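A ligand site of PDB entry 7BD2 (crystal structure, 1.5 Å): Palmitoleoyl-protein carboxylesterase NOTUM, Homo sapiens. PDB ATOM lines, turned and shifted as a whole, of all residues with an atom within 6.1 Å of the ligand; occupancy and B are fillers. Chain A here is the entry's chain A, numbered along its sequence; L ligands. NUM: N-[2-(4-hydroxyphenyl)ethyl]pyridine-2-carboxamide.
OG1 of Thr 159 is in hydrogen-bond range of O1 of the ligand. The side-chain hydroxyl (OH) of Tyr 52 is in hydrogen-bond range of an oxygen (O2) of the ligand (3.0 Å).
OG1 of Thr 159 sits at hydrogen-bond distance from O of Gly 189, at 2.9 Å. The side-chain amide oxygen (OE1) of Gln 266 sits at hydrogen-bond distance from the backbone NH (N) of Leu 192 (2.9 Å). The side-chain amide nitrogen (NE2) of Gln 266 lies within hydrogen-bond range of the side-chain amide oxygen (OD1) of Asn 194, at 3.3 Å.
Merely in contact with the ligand: Val 269, Phe 242, Phe 191, Pro 210, Val 110, Ile 214, Gln 266, Phe 243, Leu 192, Ala 156 and Ala 265. The nearest printed residue that does not touch the ligand is Trp 51 (4.2 Å).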
ATOM      1  N   TRP A  51       4.175 -10.008   0.143  1.00  0.00           N
ATOM      2  CA  TRP A  51       2.955 -10.074   0.968  1.00  0.00           C
ATOM      3  C   TRP A  51       2.743  -8.806   1.800  1.00  0.00           C
ATOM      4  O   TRP A  51       2.926  -7.704   1.275  1.00  0.00           O
ATOM      5  CB  TRP A  51       2.950 -11.348   1.813  1.00  0.00           C
ATOM      6  CG  TRP A  51       2.897 -12.582   0.917  1.00  0.00           C
ATOM      7  CD1 TRP A  51       3.958 -13.260   0.400  1.00  0.00           C
ATOM      8  CD2 TRP A  51       1.715 -13.242   0.408  1.00  0.00           C
ATOM      9  NE1 TRP A  51       3.525 -14.300  -0.373  1.00  0.00           N
ATOM     10  CE2 TRP A  51       2.156 -14.310  -0.392  1.00  0.00           C
ATOM     11  CE3 TRP A  51       0.346 -13.028   0.559  1.00  0.00           C
ATOM     12  CZ2 TRP A  51       1.274 -15.184  -1.046  1.00  0.00           C
ATOM     13  CZ3 TRP A  51      -0.540 -13.895  -0.080  1.00  0.00           C
ATOM     14  CH2 TRP A  51      -0.070 -14.955  -0.883  1.00  0.00           C
ATOM     15  N   TYR A  52       2.306  -8.939   3.056  1.00  0.00           N
ATOM     16  CA  TYR A  52       1.942  -7.819   3.921  1.00  0.00           C
ATOM     17  C   TYR A  52       1.688  -8.361   5.321  1.00  0.00           C
ATOM     18  O   TYR A  52       1.699  -9.579   5.522  1.00  0.00           O
ATOM     19  CB  TYR A  52       0.719  -7.065   3.393  1.00  0.00           C
ATOM     20  CG  TYR A  52      -0.524  -7.897   3.136  1.00  0.00           C
ATOM     21  CD1 TYR A  52      -0.734  -8.517   1.905  1.00  0.00           C
ATOM     22  CD2 TYR A  52      -1.500  -8.025   4.111  1.00  0.00           C
ATOM     23  CE1 TYR A  52      -1.893  -9.267   1.662  1.00  0.00           C
ATOM     24  CE2 TYR A  52      -2.655  -8.773   3.881  1.00  0.00           C
ATOM     25  CZ  TYR A  52      -2.845  -9.385   2.657  1.00  0.00           C
ATOM     26  OH  TYR A  52      -3.988 -10.119   2.437  1.00  0.00           O
ATOM     27  N   VAL A 110       1.237  -3.172   1.144  1.00  0.00           N
ATOM     28  CA  VAL A 110       0.908  -3.179  -0.277  1.00  0.00           C
ATOM     29  C   VAL A 110       1.054  -1.776  -0.862  1.00  0.00           C
ATOM     30  O   VAL A 110       0.335  -1.385  -1.783  1.00  0.00           O
ATOM     31  CB  VAL A 110      -0.506  -3.741  -0.560  1.00  0.00           C
ATOM     32  CG1 VAL A 110      -0.590  -4.228  -2.023  1.00  0.00           C
ATOM     33  CG2 VAL A 110      -0.860  -4.905   0.361  1.00  0.00           C
ATOM     34  N   SER A 155       4.209  -8.603  -7.761  1.00  0.00           N
ATOM     35  CA  SER A 155       3.450  -9.170  -6.621  1.00  0.00           C
ATOM     36  C   SER A 155       2.802  -8.042  -5.826  1.00  0.00           C
ATOM     37  O   SER A 155       2.065  -7.232  -6.429  1.00  0.00           O
ATOM     38  CB  SER A 155       4.408 -10.096  -5.869  1.00  0.00           C
ATOM     39  OG  SER A 155       3.722 -10.815  -4.857  1.00  0.00           O
ATOM     40  N   ALA A 156       3.046  -7.900  -4.512  1.00  0.00           N
ATOM     41  CA  ALA A 156       2.510  -6.742  -3.789  1.00  0.00           C
ATOM     42  C   ALA A 156       2.922  -5.414  -4.441  1.00  0.00           C
ATOM     43  O   ALA A 156       2.167  -4.427  -4.390  1.00  0.00           O
ATOM     44  CB  ALA A 156       2.961  -6.757  -2.317  1.00  0.00           C
ATOM     45  N   GLY A 157       4.108  -5.362  -5.080  1.00  0.00           N
ATOM     46  CA  GLY A 157       4.522  -4.169  -5.800  1.00  0.00           C
ATOM     47  C   GLY A 157       3.742  -3.944  -7.086  1.00  0.00           C
ATOM     48  O   GLY A 157       3.539  -2.800  -7.499  1.00  0.00           O
ATOM     49  N   THR A 159       0.464  -4.756  -7.400  1.00  0.00           N
ATOM     50  CA  THR A 159      -0.747  -4.100  -6.882  1.00  0.00           C
ATOM     51  C   THR A 159      -0.445  -2.647  -6.489  1.00  0.00           C
ATOM     52  O   THR A 159      -1.272  -1.745  -6.733  1.00  0.00           O
ATOM     53  CB  THR A 159      -1.308  -4.888  -5.693  1.00  0.00           C
ATOM     54  OG1 THR A 159      -1.425  -6.288  -6.029  1.00  0.00           O
ATOM     55  CG2 THR A 159      -2.681  -4.375  -5.283  1.00  0.00           C
ATOM     56  N   GLY A 160       0.744  -2.395  -5.941  1.00  0.00           N
ATOM     57  CA  GLY A 160       1.148  -1.036  -5.579  1.00  0.00           C
ATOM     58  C   GLY A 160       1.185  -0.081  -6.751  1.00  0.00           C
ATOM     59  O   GLY A 160       0.892   1.111  -6.596  1.00  0.00           O
ATOM     60  N   GLY A 189       0.249  -8.883  -9.868  1.00  0.00           N
ATOM     61  CA  GLY A 189      -0.506  -8.254  -8.811  1.00  0.00           C
ATOM     62  C   GLY A 189      -1.995  -8.141  -9.088  1.00  0.00           C
ATOM     63  O   GLY A 189      -2.686  -7.349  -8.441  1.00  0.00           O
ATOM     64  N   PHE A 191      -5.336 -10.075  -8.931  1.00  0.00           N
ATOM     65  CA  PHE A 191      -5.921 -11.232  -8.247  1.00  0.00           C
ATOM     66  C   PHE A 191      -7.449 -11.228  -8.303  1.00  0.00           C
ATOM     67  O   PHE A 191      -8.082 -10.193  -8.570  1.00  0.00           O
ATOM     68  CB  PHE A 191      -5.444 -11.280  -6.780  1.00  0.00           C
ATOM     69  CG  PHE A 191      -3.953 -11.377  -6.633  1.00  0.00           C
ATOM     70  CD1 PHE A 191      -3.227 -10.331  -6.074  1.00  0.00           C
ATOM     71  CD2 PHE A 191      -3.282 -12.490  -7.100  1.00  0.00           C
ATOM     72  CE1 PHE A 191      -1.847 -10.415  -5.958  1.00  0.00           C
ATOM     73  CE2 PHE A 191      -1.900 -12.564  -7.001  1.00  0.00           C
ATOM     74  CZ  PHE A 191      -1.187 -11.511  -6.415  1.00  0.00           C
ATOM     75  N   LEU A 192      -8.018 -12.403  -8.073  1.00  0.00           N
ATOM     76  CA  LEU A 192      -9.459 -12.622  -8.027  1.00  0.00           C
ATOM     77  C   LEU A 192      -9.920 -12.861  -6.592  1.00  0.00           C
ATOM     78  O   LEU A 192      -9.302 -13.656  -5.867  1.00  0.00           O
ATOM     79  CB  LEU A 192      -9.843 -13.820  -8.911  1.00  0.00           C
ATOM     80  CG  LEU A 192      -9.459 -13.699 -10.382  1.00  0.00           C
ATOM     81  CD1 LEU A 192      -9.872 -14.939 -11.131  1.00  0.00           C
ATOM     82  CD2 LEU A 192     -10.075 -12.455 -11.025  1.00  0.00           C
ATOM     83  N   ASP A 193     -11.021 -12.193  -6.203  1.00  0.00           N
ATOM     84  CA  ASP A 193     -11.657 -12.435  -4.911  1.00  0.00           C
ATOM     85  C   ASP A 193     -12.696 -13.561  -5.045  1.00  0.00           C
ATOM     86  O   ASP A 193     -13.913 -13.381  -4.882  1.00  0.00           O
ATOM     87  CB  ASP A 193     -12.269 -11.145  -4.342  1.00  0.00           C
ATOM     88  CG  ASP A 193     -13.145 -10.370  -5.337  1.00  0.00           C
ATOM     89  OD1 ASP A 193     -13.069 -10.590  -6.548  1.00  0.00           O
ATOM     90  OD2 ASP A 193     -13.939  -9.515  -4.866  1.00  0.00           O
ATOM     91  N   ASN A 194     -12.172 -14.756  -5.346  1.00  0.00           N
ATOM     92  CA  ASN A 194     -13.001 -15.911  -5.692  1.00  0.00           C
ATOM     93  C   ASN A 194     -13.187 -16.852  -4.508  1.00  0.00           C
ATOM     94  O   ASN A 194     -12.604 -16.681  -3.435  1.00  0.00           O
ATOM     95  CB  ASN A 194     -12.396 -16.668  -6.893  1.00  0.00           C
ATOM     96  CG  ASN A 194     -11.060 -17.335  -6.580  1.00  0.00           C
ATOM     97  OD1 ASN A 194     -10.393 -17.021  -5.597  1.00  0.00           O
ATOM     98  ND2 ASN A 194     -10.655 -18.266  -7.443  1.00  0.00           N
ATOM     99  N   PRO A 210      -8.788 -14.235   2.992  1.00  0.00           N
ATOM    100  CA  PRO A 210      -7.942 -13.198   2.391  1.00  0.00           C
ATOM    101  C   PRO A 210      -8.616 -11.828   2.377  1.00  0.00           C
ATOM    102  O   PRO A 210      -7.947 -10.830   2.653  1.00  0.00           O
ATOM    103  CB  PRO A 210      -7.726 -13.713   0.964  1.00  0.00           C
ATOM    104  N   THR A 211      -9.901 -11.775   2.044  1.00  0.00           N
ATOM    105  CA  THR A 211     -10.602 -10.492   2.057  1.00  0.00           C
ATOM    106  C   THR A 211     -10.760  -9.961   3.477  1.00  0.00           C
ATOM    107  O   THR A 211     -10.783  -8.735   3.678  1.00  0.00           O
ATOM    108  CB  THR A 211     -11.975 -10.605   1.390  1.00  0.00           C
ATOM    109  OG1 THR A 211     -12.696 -11.700   1.963  1.00  0.00           O
ATOM    110  CG2 THR A 211     -11.831 -10.812  -0.109  1.00  0.00           C
ATOM    111  N   ALA A 213      -8.461 -10.335   5.810  1.00  0.00           N
ATOM    112  CA  ALA A 213      -7.149  -9.798   6.146  1.00  0.00           C
ATOM    113  C   ALA A 213      -6.940  -8.401   5.578  1.00  0.00           C
ATOM    114  O   ALA A 213      -6.355  -7.536   6.245  1.00  0.00           O
ATOM    115  CB  ALA A 213      -6.041 -10.749   5.661  1.00  0.00           C
ATOM    116  N   ILE A 214      -7.393  -8.154   4.350  1.00  0.00           N
ATOM    117  CA  ILE A 214      -7.175  -6.828   3.764  1.00  0.00           C
ATOM    118  C   ILE A 214      -8.112  -5.806   4.385  1.00  0.00           C
ATOM    119  O   ILE A 214      -7.748  -4.626   4.541  1.00  0.00           O
ATOM    120  CB  ILE A 214      -7.306  -6.883   2.235  1.00  0.00           C
ATOM    121  CG1 ILE A 214      -6.785  -5.573   1.623  1.00  0.00           C
ATOM    122  CG2 ILE A 214      -8.737  -7.153   1.796  1.00  0.00           C
ATOM    123  CD1 ILE A 214      -5.297  -5.368   1.833  1.00  0.00           C
ATOM    124  N   TRP A 239     -11.485  -1.836   0.369  1.00  0.00           N
ATOM    125  CA  TRP A 239     -10.751  -3.073   0.084  1.00  0.00           C
ATOM    126  C   TRP A 239     -10.959  -3.537  -1.347  1.00  0.00           C
ATOM    127  O   TRP A 239     -10.090  -4.227  -1.909  1.00  0.00           O
ATOM    128  CB  TRP A 239     -11.189  -4.193   1.044  1.00  0.00           C
ATOM    129  CG  TRP A 239     -12.625  -4.699   0.814  1.00  0.00           C
ATOM    130  CD1 TRP A 239     -13.745  -4.306   1.505  1.00  0.00           C
ATOM    131  CD2 TRP A 239     -13.084  -5.661  -0.163  1.00  0.00           C
ATOM    132  NE1 TRP A 239     -14.851  -4.953   1.014  1.00  0.00           N
ATOM    133  CE2 TRP A 239     -14.482  -5.780  -0.015  1.00  0.00           C
ATOM    134  CE3 TRP A 239     -12.447  -6.419  -1.149  1.00  0.00           C
ATOM    135  CZ2 TRP A 239     -15.253  -6.636  -0.808  1.00  0.00           C
ATOM    136  CZ3 TRP A 239     -13.217  -7.270  -1.950  1.00  0.00           C
ATOM    137  CH2 TRP A 239     -14.606  -7.369  -1.777  1.00  0.00           C
ATOM    138  N   PHE A 242      -8.183  -3.015  -4.031  1.00  0.00           N
ATOM    139  CA  PHE A 242      -6.966  -3.825  -4.089  1.00  0.00           C
ATOM    140  C   PHE A 242      -7.046  -4.929  -5.134  1.00  0.00           C
ATOM    141  O   PHE A 242      -6.051  -5.609  -5.380  1.00  0.00           O
ATOM    142  CB  PHE A 242      -6.630  -4.450  -2.716  1.00  0.00           C
ATOM    143  CG  PHE A 242      -6.051  -3.479  -1.729  1.00  0.00           C
ATOM    144  CD1 PHE A 242      -4.745  -3.601  -1.282  1.00  0.00           C
ATOM    145  CD2 PHE A 242      -6.821  -2.429  -1.243  1.00  0.00           C
ATOM    146  CE1 PHE A 242      -4.224  -2.683  -0.381  1.00  0.00           C
ATOM    147  CE2 PHE A 242      -6.294  -1.504  -0.338  1.00  0.00           C
ATOM    148  CZ  PHE A 242      -4.989  -1.634   0.080  1.00  0.00           C
ATOM    149  N   PHE A 243      -8.218  -5.128  -5.754  1.00  0.00           N
ATOM    150  CA  PHE A 243      -8.373  -6.149  -6.783  1.00  0.00           C
ATOM    151  C   PHE A 243      -8.322  -5.497  -8.157  1.00  0.00           C
ATOM    152  O   PHE A 243      -9.124  -4.610  -8.454  1.00  0.00           O
ATOM    153  CB  PHE A 243      -9.665  -6.941  -6.577  1.00  0.00           C
ATOM    154  CG  PHE A 243      -9.615  -7.792  -5.342  1.00  0.00           C
ATOM    155  CD1 PHE A 243     -10.049  -7.300  -4.124  1.00  0.00           C
ATOM    156  CD2 PHE A 243      -9.032  -9.052  -5.393  1.00  0.00           C
ATOM    157  CE1 PHE A 243      -9.957  -8.087  -2.986  1.00  0.00           C
ATOM    158  CE2 PHE A 243      -8.928  -9.821  -4.254  1.00  0.00           C
ATOM    159  CZ  PHE A 243      -9.391  -9.345  -3.061  1.00  0.00           C
ATOM    160  N   ALA A 265       0.479 -17.562  -6.291  1.00  0.00           N
ATOM    161  CA  ALA A 265      -0.032 -16.969  -5.057  1.00  0.00           C
ATOM    162  C   ALA A 265      -1.545 -17.041  -5.004  1.00  0.00           C
ATOM    163  O   ALA A 265      -2.132 -17.267  -3.941  1.00  0.00           O
ATOM    164  CB  ALA A 265       0.457 -15.526  -4.915  1.00  0.00           C
ATOM    165  N   GLN A 266      -2.189 -16.900  -6.169  1.00  0.00           N
ATOM    166  CA  GLN A 266      -3.631 -17.094  -6.283  1.00  0.00           C
ATOM    167  C   GLN A 266      -4.029 -18.520  -5.887  1.00  0.00           C
ATOM    168  O   GLN A 266      -4.969 -18.721  -5.104  1.00  0.00           O
ATOM    169  CB  GLN A 266      -4.071 -16.779  -7.727  1.00  0.00           C
ATOM    170  CG  GLN A 266      -5.567 -16.964  -8.019  1.00  0.00           C
ATOM    171  CD  GLN A 266      -6.410 -15.817  -7.497  1.00  0.00           C
ATOM    172  OE1 GLN A 266      -6.128 -14.643  -7.779  1.00  0.00           O
ATOM    173  NE2 GLN A 266      -7.441 -16.135  -6.715  1.00  0.00           N
ATOM    174  N   LEU A 267      -3.303 -19.517  -6.394  1.00  0.00           N
ATOM    175  CA  LEU A 267      -3.638 -20.912  -6.076  1.00  0.00           C
ATOM    176  C   LEU A 267      -3.355 -21.234  -4.600  1.00  0.00           C
ATOM    177  O   LEU A 267      -4.075 -22.043  -4.008  1.00  0.00           O
ATOM    178  CB  LEU A 267      -2.894 -21.888  -6.990  1.00  0.00           C
ATOM    179  CG  LEU A 267      -3.414 -21.968  -8.434  1.00  0.00           C
ATOM    180  CD1 LEU A 267      -2.570 -22.891  -9.291  1.00  0.00           C
ATOM    181  CD2 LEU A 267      -4.857 -22.437  -8.455  1.00  0.00           C
ATOM    182  N   VAL A 269      -3.680 -19.110  -1.935  1.00  0.00           N
ATOM    183  CA  VAL A 269      -4.793 -18.623  -1.129  1.00  0.00           C
ATOM    184  C   VAL A 269      -6.088 -19.351  -1.471  1.00  0.00           C
ATOM    185  O   VAL A 269      -7.002 -19.388  -0.634  1.00  0.00           O
ATOM    186  CB  VAL A 269      -4.981 -17.103  -1.268  1.00  0.00           C
ATOM    187  CG1 VAL A 269      -3.694 -16.361  -0.895  1.00  0.00           C
ATOM    188  CG2 VAL A 269      -5.457 -16.756  -2.650  1.00  0.00           C
HETATM  189  N1  NUM L   1      -6.269 -10.472  -1.252  1.00  0.00           N
HETATM  190  C4  NUM L   1      -4.988  -7.928  -1.798  1.00  0.00           C
HETATM  191  C5  NUM L   1      -6.355  -8.086  -1.107  1.00  0.00           C
HETATM  192  C6  NUM L   1      -6.548  -9.398  -0.321  1.00  0.00           C
HETATM  193  C7  NUM L   1      -5.077 -11.277  -1.182  1.00  0.00           C
HETATM  194  C8  NUM L   1      -4.955 -12.310  -2.297  1.00  0.00           C
HETATM  195  C10 NUM L   1      -6.007 -13.552  -4.015  1.00  0.00           C
HETATM  196  C13 NUM L   1      -4.882  -7.871  -3.180  1.00  0.00           C
HETATM  197  C1  NUM L   1      -2.504  -7.612  -3.004  1.00  0.00           C
HETATM  198  C11 NUM L   1      -4.762 -14.075  -4.320  1.00  0.00           C
HETATM  199  C12 NUM L   1      -3.657 -13.695  -3.578  1.00  0.00           C
HETATM  200  C14 NUM L   1      -3.646  -7.720  -3.788  1.00  0.00           C
HETATM  201  C2  NUM L   1      -2.603  -7.657  -1.625  1.00  0.00           C
HETATM  202  C3  NUM L   1      -3.838  -7.826  -1.016  1.00  0.00           C
HETATM  203  C9  NUM L   1      -6.103 -12.630  -2.986  1.00  0.00           C
HETATM  204  N2  NUM L   1      -3.769 -12.813  -2.599  1.00  0.00           N
HETATM  205  O1  NUM L   1      -1.242  -7.446  -3.599  1.00  0.00           O
HETATM  206  O2  NUM L   1      -4.241 -11.123  -0.366  1.00  0.00           O
